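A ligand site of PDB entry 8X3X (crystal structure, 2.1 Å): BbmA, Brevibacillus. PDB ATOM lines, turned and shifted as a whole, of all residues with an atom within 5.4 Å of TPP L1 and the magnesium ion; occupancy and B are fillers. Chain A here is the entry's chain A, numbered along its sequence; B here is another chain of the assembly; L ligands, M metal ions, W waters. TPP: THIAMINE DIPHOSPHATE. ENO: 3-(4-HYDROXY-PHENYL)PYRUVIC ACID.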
ATOM      1  N   ASN A 399     -15.319 -13.648 -14.186  1.00  0.00           N
ATOM      2  CA  ASN A 399     -14.798 -13.063 -12.973  1.00  0.00           C
ATOM      3  C   ASN A 399     -15.922 -13.012 -11.951  1.00  0.00           C
ATOM      4  O   ASN A 399     -17.020 -12.531 -12.256  1.00  0.00           O
ATOM      5  CB  ASN A 399     -14.199 -11.686 -13.289  1.00  0.00           C
ATOM      6  CG  ASN A 399     -13.036 -11.786 -14.303  1.00  0.00           C
ATOM      7  OD1 ASN A 399     -11.959 -12.306 -13.982  1.00  0.00           O
ATOM      8  ND2 ASN A 399     -13.267 -11.298 -15.536  1.00  0.00           N
ATOM      9  N   GLY A 400     -15.657 -13.512 -10.764  1.00  0.00           N
ATOM     10  CA  GLY A 400     -16.633 -13.975  -9.797  1.00  0.00           C
ATOM     11  C   GLY A 400     -16.100 -15.254  -9.200  1.00  0.00           C
ATOM     12  O   GLY A 400     -14.948 -15.633  -9.430  1.00  0.00           O
ATOM     13  N   SER A 401     -16.952 -15.960  -8.432  1.00  0.00           N
ATOM     14  CA  SER A 401     -16.525 -17.221  -7.845  1.00  0.00           C
ATOM     15  C   SER A 401     -16.079 -18.224  -8.899  1.00  0.00           C
ATOM     16  O   SER A 401     -15.370 -19.179  -8.566  1.00  0.00           O
ATOM     17  CB  SER A 401     -17.649 -17.836  -7.005  1.00  0.00           C
ATOM     18  OG  SER A 401     -18.628 -18.442  -7.838  1.00  0.00           O
ATOM     19  N   CYS A 402     -16.485 -18.040 -10.158  1.00  0.00           N
ATOM     20  CA  CYS A 402     -16.003 -18.925 -11.216  1.00  0.00           C
ATOM     21  C   CYS A 402     -14.483 -18.873 -11.356  1.00  0.00           C
ATOM     22  O   CYS A 402     -13.864 -19.861 -11.764  1.00  0.00           O
ATOM     23  CB  CYS A 402     -16.696 -18.582 -12.531  1.00  0.00           C
ATOM     24  SG  CYS A 402     -16.395 -16.905 -13.085  1.00  0.00           S
ATOM     25  N   LEU A 424      -7.634  -7.094 -15.305  1.00  0.00           N
ATOM     26  CA  LEU A 424      -8.663  -6.213 -14.770  1.00  0.00           C
ATOM     27  C   LEU A 424      -9.811  -6.978 -14.143  1.00  0.00           C
ATOM     28  O   LEU A 424     -10.569  -6.398 -13.358  1.00  0.00           O
ATOM     29  CB  LEU A 424      -9.211  -5.302 -15.881  1.00  0.00           C
ATOM     30  CG  LEU A 424      -9.696  -3.896 -15.529  1.00  0.00           C
ATOM     31  CD1 LEU A 424      -8.698  -3.149 -14.650  1.00  0.00           C
ATOM     32  CD2 LEU A 424      -9.958  -3.134 -16.801  1.00  0.00           C
ATOM     33  N   ALA A 425      -9.958  -8.261 -14.461  1.00  0.00           N
ATOM     34  CA  ALA A 425     -10.994  -9.119 -13.877  1.00  0.00           C
ATOM     35  C   ALA A 425     -12.371  -8.462 -13.998  1.00  0.00           C
ATOM     36  O   ALA A 425     -13.113  -8.315 -13.019  1.00  0.00           O
ATOM     37  CB  ALA A 425     -10.670  -9.467 -12.419  1.00  0.00           C
ATOM     38  N   ALA A 426     -12.714  -8.069 -15.207  1.00  0.00           N
ATOM     39  CA  ALA A 426     -13.983  -7.400 -15.455  1.00  0.00           C
ATOM     40  C   ALA A 426     -15.080  -8.429 -15.580  1.00  0.00           C
ATOM     41  O   ALA A 426     -14.973  -9.377 -16.368  1.00  0.00           O
ATOM     42  CB  ALA A 426     -13.886  -6.549 -16.720  1.00  0.00           C
ATOM     43  N   MET A 427     -16.149  -8.255 -14.799  1.00  0.00           N
ATOM     44  CA  MET A 427     -17.324  -9.106 -14.962  1.00  0.00           C
ATOM     45  C   MET A 427     -17.830  -9.005 -16.381  1.00  0.00           C
ATOM     46  O   MET A 427     -17.893  -7.917 -16.952  1.00  0.00           O
ATOM     47  CB  MET A 427     -18.427  -8.684 -14.003  1.00  0.00           C
ATOM     48  CG  MET A 427     -18.210  -9.154 -12.605  1.00  0.00           C
ATOM     49  SD  MET A 427     -19.458  -8.404 -11.566  1.00  0.00           S
ATOM     50  CE  MET A 427     -20.982  -9.022 -12.304  1.00  0.00           C
ATOM     51  N   GLY A 451     -20.610 -16.457 -14.111  1.00  0.00           N
ATOM     52  CA  GLY A 451     -21.641 -16.249 -13.102  1.00  0.00           C
ATOM     53  C   GLY A 451     -22.896 -15.567 -13.665  1.00  0.00           C
ATOM     54  O   GLY A 451     -22.897 -15.057 -14.788  1.00  0.00           O
ATOM     55  N   ASP A 452     -23.951 -15.557 -12.852  1.00  0.00           N
ATOM     56  CA  ASP A 452     -25.236 -15.027 -13.328  1.00  0.00           C
ATOM     57  C   ASP A 452     -25.224 -13.506 -13.415  1.00  0.00           C
ATOM     58  O   ASP A 452     -25.803 -12.939 -14.355  1.00  0.00           O
ATOM     59  CB  ASP A 452     -26.389 -15.514 -12.447  1.00  0.00           C
ATOM     60  CG  ASP A 452     -26.232 -15.165 -10.955  1.00  0.00           C
ATOM     61  OD1 ASP A 452     -25.194 -15.489 -10.351  1.00  0.00           O
ATOM     62  OD2 ASP A 452     -27.181 -14.592 -10.396  1.00  0.00           O
ATOM     63  N   ALA A 453     -24.585 -12.833 -12.453  1.00  0.00           N
ATOM     64  CA  ALA A 453     -24.527 -11.369 -12.534  1.00  0.00           C
ATOM     65  C   ALA A 453     -23.672 -10.922 -13.715  1.00  0.00           C
ATOM     66  O   ALA A 453     -24.007  -9.936 -14.394  1.00  0.00           O
ATOM     67  CB  ALA A 453     -23.997 -10.772 -11.242  1.00  0.00           C
ATOM     68  N   ALA A 454     -22.566 -11.616 -13.958  1.00  0.00           N
ATOM     69  CA  ALA A 454     -21.760 -11.323 -15.142  1.00  0.00           C
ATOM     70  C   ALA A 454     -22.574 -11.518 -16.417  1.00  0.00           C
ATOM     71  O   ALA A 454     -22.449 -10.724 -17.367  1.00  0.00           O
ATOM     72  CB  ALA A 454     -20.513 -12.205 -15.166  1.00  0.00           C
ATOM     73  N   PHE A 455     -23.406 -12.566 -16.460  1.00  0.00           N
ATOM     74  CA  PHE A 455     -24.211 -12.808 -17.647  1.00  0.00           C
ATOM     75  C   PHE A 455     -25.283 -11.736 -17.812  1.00  0.00           C
ATOM     76  O   PHE A 455     -25.583 -11.315 -18.941  1.00  0.00           O
ATOM     77  CB  PHE A 455     -24.844 -14.199 -17.608  1.00  0.00           C
ATOM     78  CG  PHE A 455     -25.289 -14.689 -18.954  1.00  0.00           C
ATOM     79  CD1 PHE A 455     -24.402 -15.359 -19.785  1.00  0.00           C
ATOM     80  CD2 PHE A 455     -26.587 -14.470 -19.399  1.00  0.00           C
ATOM     81  CE1 PHE A 455     -24.793 -15.788 -21.035  1.00  0.00           C
ATOM     82  CE2 PHE A 455     -26.995 -14.913 -20.653  1.00  0.00           C
ATOM     83  CZ  PHE A 455     -26.081 -15.578 -21.468  1.00  0.00           C
ATOM     84  N   MET A 457     -24.712  -8.835 -17.265  1.00  0.00           N
ATOM     85  CA  MET A 457     -23.985  -7.651 -17.703  1.00  0.00           C
ATOM     86  C   MET A 457     -23.692  -7.659 -19.199  1.00  0.00           C
ATOM     87  O   MET A 457     -23.782  -6.615 -19.841  1.00  0.00           O
ATOM     88  CB  MET A 457     -22.684  -7.533 -16.904  1.00  0.00           C
ATOM     89  CG  MET A 457     -22.371  -6.152 -16.411  1.00  0.00           C
ATOM     90  SD  MET A 457     -20.889  -6.190 -15.378  1.00  0.00           S
ATOM     91  CE  MET A 457     -21.558  -6.227 -13.719  1.00  0.00           C
ATOM     92  N   LEU A 477     -23.328 -20.275 -13.787  1.00  0.00           N
ATOM     93  CA  LEU A 477     -23.468 -20.703 -12.405  1.00  0.00           C
ATOM     94  C   LEU A 477     -24.475 -19.767 -11.753  1.00  0.00           C
ATOM     95  O   LEU A 477     -24.133 -18.668 -11.294  1.00  0.00           O
ATOM     96  CB  LEU A 477     -22.138 -20.675 -11.673  1.00  0.00           C
ATOM     97  CG  LEU A 477     -20.977 -21.583 -12.139  1.00  0.00           C
ATOM     98  CD1 LEU A 477     -19.767 -21.306 -11.268  1.00  0.00           C
ATOM     99  CD2 LEU A 477     -21.315 -23.078 -12.106  1.00  0.00           C
ATOM    100  N   ASN A 479     -26.454 -18.611  -9.012  1.00  0.00           N
ATOM    101  CA  ASN A 479     -26.680 -18.651  -7.571  1.00  0.00           C
ATOM    102  C   ASN A 479     -27.551 -17.500  -7.082  1.00  0.00           C
ATOM    103  O   ASN A 479     -27.599 -17.235  -5.879  1.00  0.00           O
ATOM    104  CB  ASN A 479     -25.342 -18.691  -6.819  1.00  0.00           C
ATOM    105  CG  ASN A 479     -24.430 -17.557  -7.180  1.00  0.00           C
ATOM    106  OD1 ASN A 479     -24.846 -16.581  -7.797  1.00  0.00           O
ATOM    107  ND2 ASN A 479     -23.163 -17.666  -6.775  1.00  0.00           N
ATOM    108  N   GLY A 480     -28.232 -16.812  -7.995  1.00  0.00           N
ATOM    109  CA  GLY A 480     -29.194 -15.778  -7.621  1.00  0.00           C
ATOM    110  C   GLY A 480     -28.570 -14.527  -7.051  1.00  0.00           C
ATOM    111  O   GLY A 480     -29.081 -13.981  -6.056  1.00  0.00           O
ATOM    112  N   GLY A 481     -27.461 -14.063  -7.626  1.00  0.00           N
ATOM    113  CA  GLY A 481     -26.883 -12.807  -7.206  1.00  0.00           C
ATOM    114  C   GLY A 481     -25.366 -12.855  -7.209  1.00  0.00           C
ATOM    115  O   GLY A 481     -24.743 -13.653  -7.912  1.00  0.00           O
ATOM    116  N   HIS A 482     -24.781 -11.955  -6.425  1.00  0.00           N
ATOM    117  CA  HIS A 482     -23.334 -11.737  -6.372  1.00  0.00           C
ATOM    118  C   HIS A 482     -22.749 -12.585  -5.264  1.00  0.00           C
ATOM    119  O   HIS A 482     -22.647 -12.155  -4.108  1.00  0.00           O
ATOM    120  CB  HIS A 482     -23.039 -10.255  -6.171  1.00  0.00           C
ATOM    121  CG  HIS A 482     -23.591  -9.375  -7.240  1.00  0.00           C
ATOM    122  ND1 HIS A 482     -22.792  -8.659  -8.105  1.00  0.00           N
ATOM    123  CD2 HIS A 482     -24.869  -9.083  -7.595  1.00  0.00           C
ATOM    124  CE1 HIS A 482     -23.550  -7.960  -8.925  1.00  0.00           C
ATOM    125  NE2 HIS A 482     -24.814  -8.198  -8.643  1.00  0.00           N
ATOM    126  N   GLY A 483     -22.311 -13.797  -5.615  1.00  0.00           N
ATOM    127  CA  GLY A 483     -21.856 -14.748  -4.603  1.00  0.00           C
ATOM    128  C   GLY A 483     -20.658 -14.234  -3.815  1.00  0.00           C
ATOM    129  O   GLY A 483     -20.668 -14.251  -2.575  1.00  0.00           O
ATOM    130  N   LEU A 484     -19.618 -13.779  -4.520  1.00  0.00           N
ATOM    131  CA  LEU A 484     -18.440 -13.287  -3.810  1.00  0.00           C
ATOM    132  C   LEU A 484     -18.793 -12.151  -2.866  1.00  0.00           C
ATOM    133  O   LEU A 484     -18.287 -12.097  -1.731  1.00  0.00           O
ATOM    134  CB  LEU A 484     -17.371 -12.854  -4.808  1.00  0.00           C
ATOM    135  CG  LEU A 484     -16.673 -13.970  -5.604  1.00  0.00           C
ATOM    136  CD1 LEU A 484     -15.353 -13.444  -6.206  1.00  0.00           C
ATOM    137  CD2 LEU A 484     -16.425 -15.212  -4.755  1.00  0.00           C
ATOM    138  N   VAL A 485     -19.654 -11.224  -3.291  1.00  0.00           N
ATOM    139  CA  VAL A 485     -20.040 -10.114  -2.408  1.00  0.00           C
ATOM    140  C   VAL A 485     -20.823 -10.636  -1.222  1.00  0.00           C
ATOM    141  O   VAL A 485     -20.604 -10.207  -0.079  1.00  0.00           O
ATOM    142  CB  VAL A 485     -20.852  -9.051  -3.174  1.00  0.00           C
ATOM    143  CG1 VAL A 485     -21.221  -7.895  -2.210  1.00  0.00           C
ATOM    144  CG2 VAL A 485     -20.103  -8.538  -4.382  1.00  0.00           C
ATOM    145  N   ILE B  28     -22.997  -0.912  -8.215  1.00  0.00           N
ATOM    146  CA  ILE B  28     -22.702  -2.332  -8.043  1.00  0.00           C
ATOM    147  C   ILE B  28     -21.530  -2.413  -7.067  1.00  0.00           C
ATOM    148  O   ILE B  28     -20.492  -1.751  -7.278  1.00  0.00           O
ATOM    149  CB  ILE B  28     -22.359  -3.008  -9.384  1.00  0.00           C
ATOM    150  CG1 ILE B  28     -23.548  -2.930 -10.356  1.00  0.00           C
ATOM    151  CG2 ILE B  28     -21.932  -4.459  -9.173  1.00  0.00           C
ATOM    152  CD1 ILE B  28     -23.222  -3.296 -11.808  1.00  0.00           C
ATOM    153  N   PRO B  29     -21.633  -3.193  -6.005  1.00  0.00           N
ATOM    154  CA  PRO B  29     -20.548  -3.244  -5.021  1.00  0.00           C
ATOM    155  C   PRO B  29     -19.290  -3.902  -5.564  1.00  0.00           C
ATOM    156  O   PRO B  29     -19.263  -4.518  -6.637  1.00  0.00           O
ATOM    157  CB  PRO B  29     -21.149  -4.075  -3.870  1.00  0.00           C
ATOM    158  CG  PRO B  29     -22.131  -4.970  -4.585  1.00  0.00           C
ATOM    159  CD  PRO B  29     -22.754  -4.076  -5.637  1.00  0.00           C
ATOM    160  N   GLY B  30     -18.222  -3.738  -4.788  1.00  0.00           N
ATOM    161  CA  GLY B  30     -16.945  -4.410  -5.002  1.00  0.00           C
ATOM    162  C   GLY B  30     -16.178  -4.349  -3.701  1.00  0.00           C
ATOM    163  O   GLY B  30     -16.462  -3.514  -2.839  1.00  0.00           O
ATOM    164  N   GLU B  54     -22.848  -1.062 -14.408  1.00  0.00           N
ATOM    165  CA  GLU B  54     -22.560   0.262 -13.849  1.00  0.00           C
ATOM    166  C   GLU B  54     -22.919   1.374 -14.831  1.00  0.00           C
ATOM    167  O   GLU B  54     -23.159   2.511 -14.416  1.00  0.00           O
ATOM    168  CB  GLU B  54     -21.089   0.381 -13.447  1.00  0.00           C
ATOM    169  CG  GLU B  54     -20.737  -0.468 -12.263  1.00  0.00           C
ATOM    170  CD  GLU B  54     -20.232  -1.852 -12.669  1.00  0.00           C
ATOM    171  OE1 GLU B  54     -19.637  -2.518 -11.807  1.00  0.00           O
ATOM    172  OE2 GLU B  54     -20.443  -2.270 -13.827  1.00  0.00           O
ATOM    173  N   THR B  77     -16.827   0.039  -8.259  1.00  0.00           N
ATOM    174  CA  THR B  77     -15.596  -0.461  -7.681  1.00  0.00           C
ATOM    175  C   THR B  77     -14.395  -0.051  -8.529  1.00  0.00           C
ATOM    176  O   THR B  77     -14.508   0.666  -9.526  1.00  0.00           O
ATOM    177  CB  THR B  77     -15.646  -1.983  -7.520  1.00  0.00           C
ATOM    178  OG1 THR B  77     -14.576  -2.397  -6.662  1.00  0.00           O
ATOM    179  CG2 THR B  77     -15.537  -2.697  -8.890  1.00  0.00           C
ATOM    180  N   PRO B  80     -12.640  -2.054 -13.635  1.00  0.00           N
ATOM    181  CA  PRO B  80     -13.712  -2.206 -14.642  1.00  0.00           C
ATOM    182  C   PRO B  80     -15.079  -1.759 -14.145  1.00  0.00           C
ATOM    183  O   PRO B  80     -15.944  -1.432 -14.971  1.00  0.00           O
ATOM    184  CB  PRO B  80     -13.696  -3.709 -14.939  1.00  0.00           C
ATOM    185  CG  PRO B  80     -13.266  -4.333 -13.620  1.00  0.00           C
ATOM    186  CD  PRO B  80     -12.243  -3.345 -13.044  1.00  0.00           C
ATOM    187  N   GLY B  81     -15.330  -1.751 -12.840  1.00  0.00           N
ATOM    188  CA  GLY B  81     -16.565  -1.166 -12.352  1.00  0.00           C
ATOM    189  C   GLY B  81     -16.690   0.284 -12.793  1.00  0.00           C
ATOM    190  O   GLY B  81     -17.679   0.675 -13.431  1.00  0.00           O
ATOM    191  N   ASN B  84     -16.919   0.933 -16.620  1.00  0.00           N
ATOM    192  CA  ASN B  84     -18.250   0.611 -17.118  1.00  0.00           C
ATOM    193  C   ASN B  84     -19.220   1.783 -16.991  1.00  0.00           C
ATOM    194  O   ASN B  84     -20.201   1.853 -17.728  1.00  0.00           O
ATOM    195  CB  ASN B  84     -18.844  -0.593 -16.356  1.00  0.00           C
ATOM    196  CG  ASN B  84     -18.571  -1.930 -17.060  1.00  0.00           C
ATOM    197  OD1 ASN B  84     -17.941  -1.980 -18.100  1.00  0.00           O
ATOM    198  ND2 ASN B  84     -19.071  -3.021 -16.477  1.00  0.00           N
ATOM    199  N   GLN B 117      -6.963  -4.884  -9.739  1.00  0.00           N
ATOM    200  CA  GLN B 117      -7.696  -3.791 -10.366  1.00  0.00           C
ATOM    201  C   GLN B 117      -7.098  -2.430 -10.006  1.00  0.00           C
ATOM    202  O   GLN B 117      -7.804  -1.426  -9.905  1.00  0.00           O
ATOM    203  CB  GLN B 117      -9.185  -3.855 -10.008  1.00  0.00           C
ATOM    204  CG  GLN B 117      -9.864  -5.170 -10.491  1.00  0.00           C
ATOM    205  CD  GLN B 117     -11.328  -5.283 -10.077  1.00  0.00           C
ATOM    206  OE1 GLN B 117     -11.750  -4.659  -9.117  1.00  0.00           O
ATOM    207  NE2 GLN B 117     -12.102  -6.091 -10.817  1.00  0.00           N
HETATM  208  N1' TPP L   1     -18.186  -4.692 -11.582  1.00  0.00           N
HETATM  209  C2' TPP L   1     -17.408  -5.208 -12.563  1.00  0.00           C
HETATM  210  CM2 TPP L   1     -17.660  -4.719 -13.951  1.00  0.00           C
HETATM  211  N3' TPP L   1     -16.439  -6.110 -12.400  1.00  0.00           N
HETATM  212  C4' TPP L   1     -16.211  -6.562 -11.156  1.00  0.00           C
HETATM  213  N4' TPP L   1     -15.222  -7.456 -11.005  1.00  0.00           N
HETATM  214  C5' TPP L   1     -16.968  -6.081 -10.045  1.00  0.00           C
HETATM  215  C6' TPP L   1     -17.941  -5.153 -10.350  1.00  0.00           C
HETATM  216  C7' TPP L   1     -16.755  -6.556  -8.639  1.00  0.00           C
HETATM  217  N3  TPP L   1     -17.127  -7.975  -8.460  1.00  0.00           N
HETATM  218  C2  TPP L   1     -16.259  -8.962  -8.407  1.00  0.00           C
HETATM  219  S1  TPP L   1     -17.002 -10.455  -8.229  1.00  0.00           S
HETATM  220  C5  TPP L   1     -18.562  -9.711  -8.227  1.00  0.00           C
HETATM  221  C4  TPP L   1     -18.466  -8.382  -8.388  1.00  0.00           C
HETATM  222  CM4 TPP L   1     -19.574  -7.401  -8.452  1.00  0.00           C
HETATM  223  C6  TPP L   1     -19.792 -10.566  -8.181  1.00  0.00           C
HETATM  224  C7  TPP L   1     -19.875 -11.458  -9.401  1.00  0.00           C
HETATM  225  O7  TPP L   1     -21.142 -12.161  -9.419  1.00  0.00           O
HETATM  226  PA  TPP L   1     -21.456 -13.327 -10.431  1.00  0.00           P
HETATM  227  O1A TPP L   1     -21.025 -13.062 -11.823  1.00  0.00           O
HETATM  228  O2A TPP L   1     -22.928 -13.738 -10.292  1.00  0.00           O
HETATM  229  O3A TPP L   1     -20.584 -14.469  -9.774  1.00  0.00           O
HETATM  230  PB  TPP L   1     -20.555 -15.350  -8.446  1.00  0.00           P
HETATM  231  O1B TPP L   1     -20.201 -16.770  -8.776  1.00  0.00           O
HETATM  232  O2B TPP L   1     -21.971 -15.157  -7.853  1.00  0.00           O
HETATM  233  O3B TPP L   1     -19.575 -14.636  -7.508  1.00  0.00           O
HETATM  234  O4  ENO L   2     -15.267  -7.399  -5.916  1.00  0.00           O
HETATM  235  C9  ENO L   2     -14.913  -9.549  -2.294  1.00  0.00           C
HETATM  236  C8  ENO L   2     -15.108  -9.194  -0.961  1.00  0.00           C
HETATM  237  C7  ENO L   2     -16.143  -8.333  -0.601  1.00  0.00           C
HETATM  238  C6  ENO L   2     -17.000  -7.829  -1.572  1.00  0.00           C
HETATM  239  C5  ENO L   2     -16.819  -8.200  -2.896  1.00  0.00           C
HETATM  240  C4  ENO L   2     -15.790  -9.054  -3.254  1.00  0.00           C
HETATM  241  O3  ENO L   2     -16.337  -7.966   0.741  1.00  0.00           O
HETATM  242  C3  ENO L   2     -15.604  -9.400  -4.730  1.00  0.00           C
HETATM  243  C2  ENO L   2     -14.756  -8.283  -5.318  1.00  0.00           C
HETATM  244  C1  ENO L   2     -13.252  -8.293  -5.075  1.00  0.00           C
HETATM  245  O2  ENO L   2     -12.627  -7.215  -4.975  1.00  0.00           O
HETATM  246  O1  ENO L   2     -12.634  -9.390  -4.954  1.00  0.00           O
HETATM  247 MG    MG M   1     -23.741 -15.103  -9.022  1.00  0.00          MG
HETATM  248  O   HOH W   1     -18.868 -16.865 -11.243  1.00  0.00           O
HETATM  249  O   HOH W   2     -22.778 -16.794 -10.007  1.00  0.00           O
HETATM  250  O   HOH W   3     -18.984 -14.451 -13.078  1.00  0.00           O
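An oxygen (O2A) of TPP L1 lies close to the backbone NH (N) of Asp 452, at 3.3 Å. The backbone NH of Ser 401 is in hydrogen-bond range of an oxygen (O3B) of TPP L1 (3.1 Å). O1B of TPP L1 lies within hydrogen-bond range of OG of Ser 401 (2.5 Å). OE1 of Glu 54 of chain B lies within hydrogen-bond range of N1' of TPP L1 (2.6 Å). An oxygen (O3B) of TPP L1 lies within hydrogen-bond range of the backbone NH (N) of Gly 483, at 3.4 Å. N of Ala 453 sits close to O2A of TPP L1 (2.9 Å). O1A of TPP L1 is in hydrogen-bond range of N of Ala 454, at 3.0 Å. A nitrogen (N4') of TPP L1 sits at hydrogen-bond distance from the backbone carbonyl oxygen (O) of Ala 425 (3.0 Å). The backbone NH of Leu 484 lies within hydrogen-bond range of an oxygen (O3B) of TPP L1 (3.1 Å). A nitrogen (N3') of TPP L1 lies within hydrogen-bond range of the backbone NH (N) of Met 427 (3.2 Å). The side-chain amide nitrogen (NE2) of Gln 117 of chain B lies close to a nitrogen (N4') of TPP L1 (3.4 Å).
N of Asp 452 lies within hydrogen-bond range of O of Leu 477 (3.5 Å). The side-chain carboxylate (OD2) of Asp 452 sits at hydrogen-bond distance from the backbone NH (N) of Gly 480, at 3.4 Å. The side-chain carboxylate (OE2) of Glu 54 of chain B is in hydrogen-bond range of the side-chain amide nitrogen (ND2) of Asn 84 of chain B (3.1 Å). O of Ala 425 lies within hydrogen-bond range of NE2 of Gln 117 of chain B (3.3 Å). NE2 of Gln 117 of chain B lies within hydrogen-bond range of O of Leu 424.
Gly 400 touches TPP L1 (CA to O3B, 3.8 Å). Gly 451 touches TPP L1. Met 457 touches TPP L1 (SD to CM2, 3.8 Å). ND1 of His 482 touches CM4 of TPP L1, at 3.5 Å. CG2 of Ile 28 of chain B touches CM4 of TPP L1 (3.8 Å). Pro 29 of chain B touches TPP L1. CG2 of Thr 77 of chain B touches C6' of TPP L1, 3.7 Å away. Pro 80 of chain B touches TPP L1 (CG to N3', 3.8 Å). Gly 81 of chain B touches TPP L1. Asn 84 of chain B touches TPP L1. Hydrophobic or aromatic side chains that line TPP L1: Met 427, Ala 453, Ala 454, Met 457, His 482, Leu 484, Ile 28 of chain B and Pro 80 of chain B. Within 4 Å of TPP L1: Gly 400, Ser 401, Ala 425, Met 427, Gly 451, Asp 452, Ala 453, Ala 454, Met 457, Asn 479, Gly 481, His 482, Gly 483, Leu 484, Ile 28 of chain B, Pro 29 of chain B, Glu 54 of chain B, Thr 77 of chain B, Pro 80 of chain B, Gly 81 of chain B, Asn 84 of chain B and Gln 117 of chain B. The nearest printed residue that does not touch TPP L1 is Asn 399 (4.1 Å).
Merely in contact with the magnesium ion: Gly 483 (3.9 Å). Of the 31 residues printed, 4 come within 4 Å of the magnesium ion.
The magnesium ion is bound by OD1 of Asp 452, 2.0 Å away. O2A of TPP L1 binds the magnesium ion. The magnesium ion is bound by O of Gly 481. The magnesium ion is bound by an oxygen (O2B) of TPP L1 (2.1 Å). Water W2 binds the magnesium ion. OD1 of Asn 479 binds the magnesium ion, 2.2 Å away.
Water W2 lies within hydrogen-bond range of O of Leu 477 (2.6 Å), O1B of TPP L1 (2.9 Å), N of Asp 452 (3.3 Å) and ND2 of Asn 479 (3.4 Å). Water W3 lies within hydrogen-bond range of O1A of TPP L1, N of Gly 451, O of Asn 399 and SG of Cys 402. Water W1 lies within hydrogen-bond range of an oxygen (O1B) of TPP L1 (2.8 Å), the backbone NH (N) of Cys 402 (2.9 Å) and the backbone NH (N) of Gly 451 (3.4 Å).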
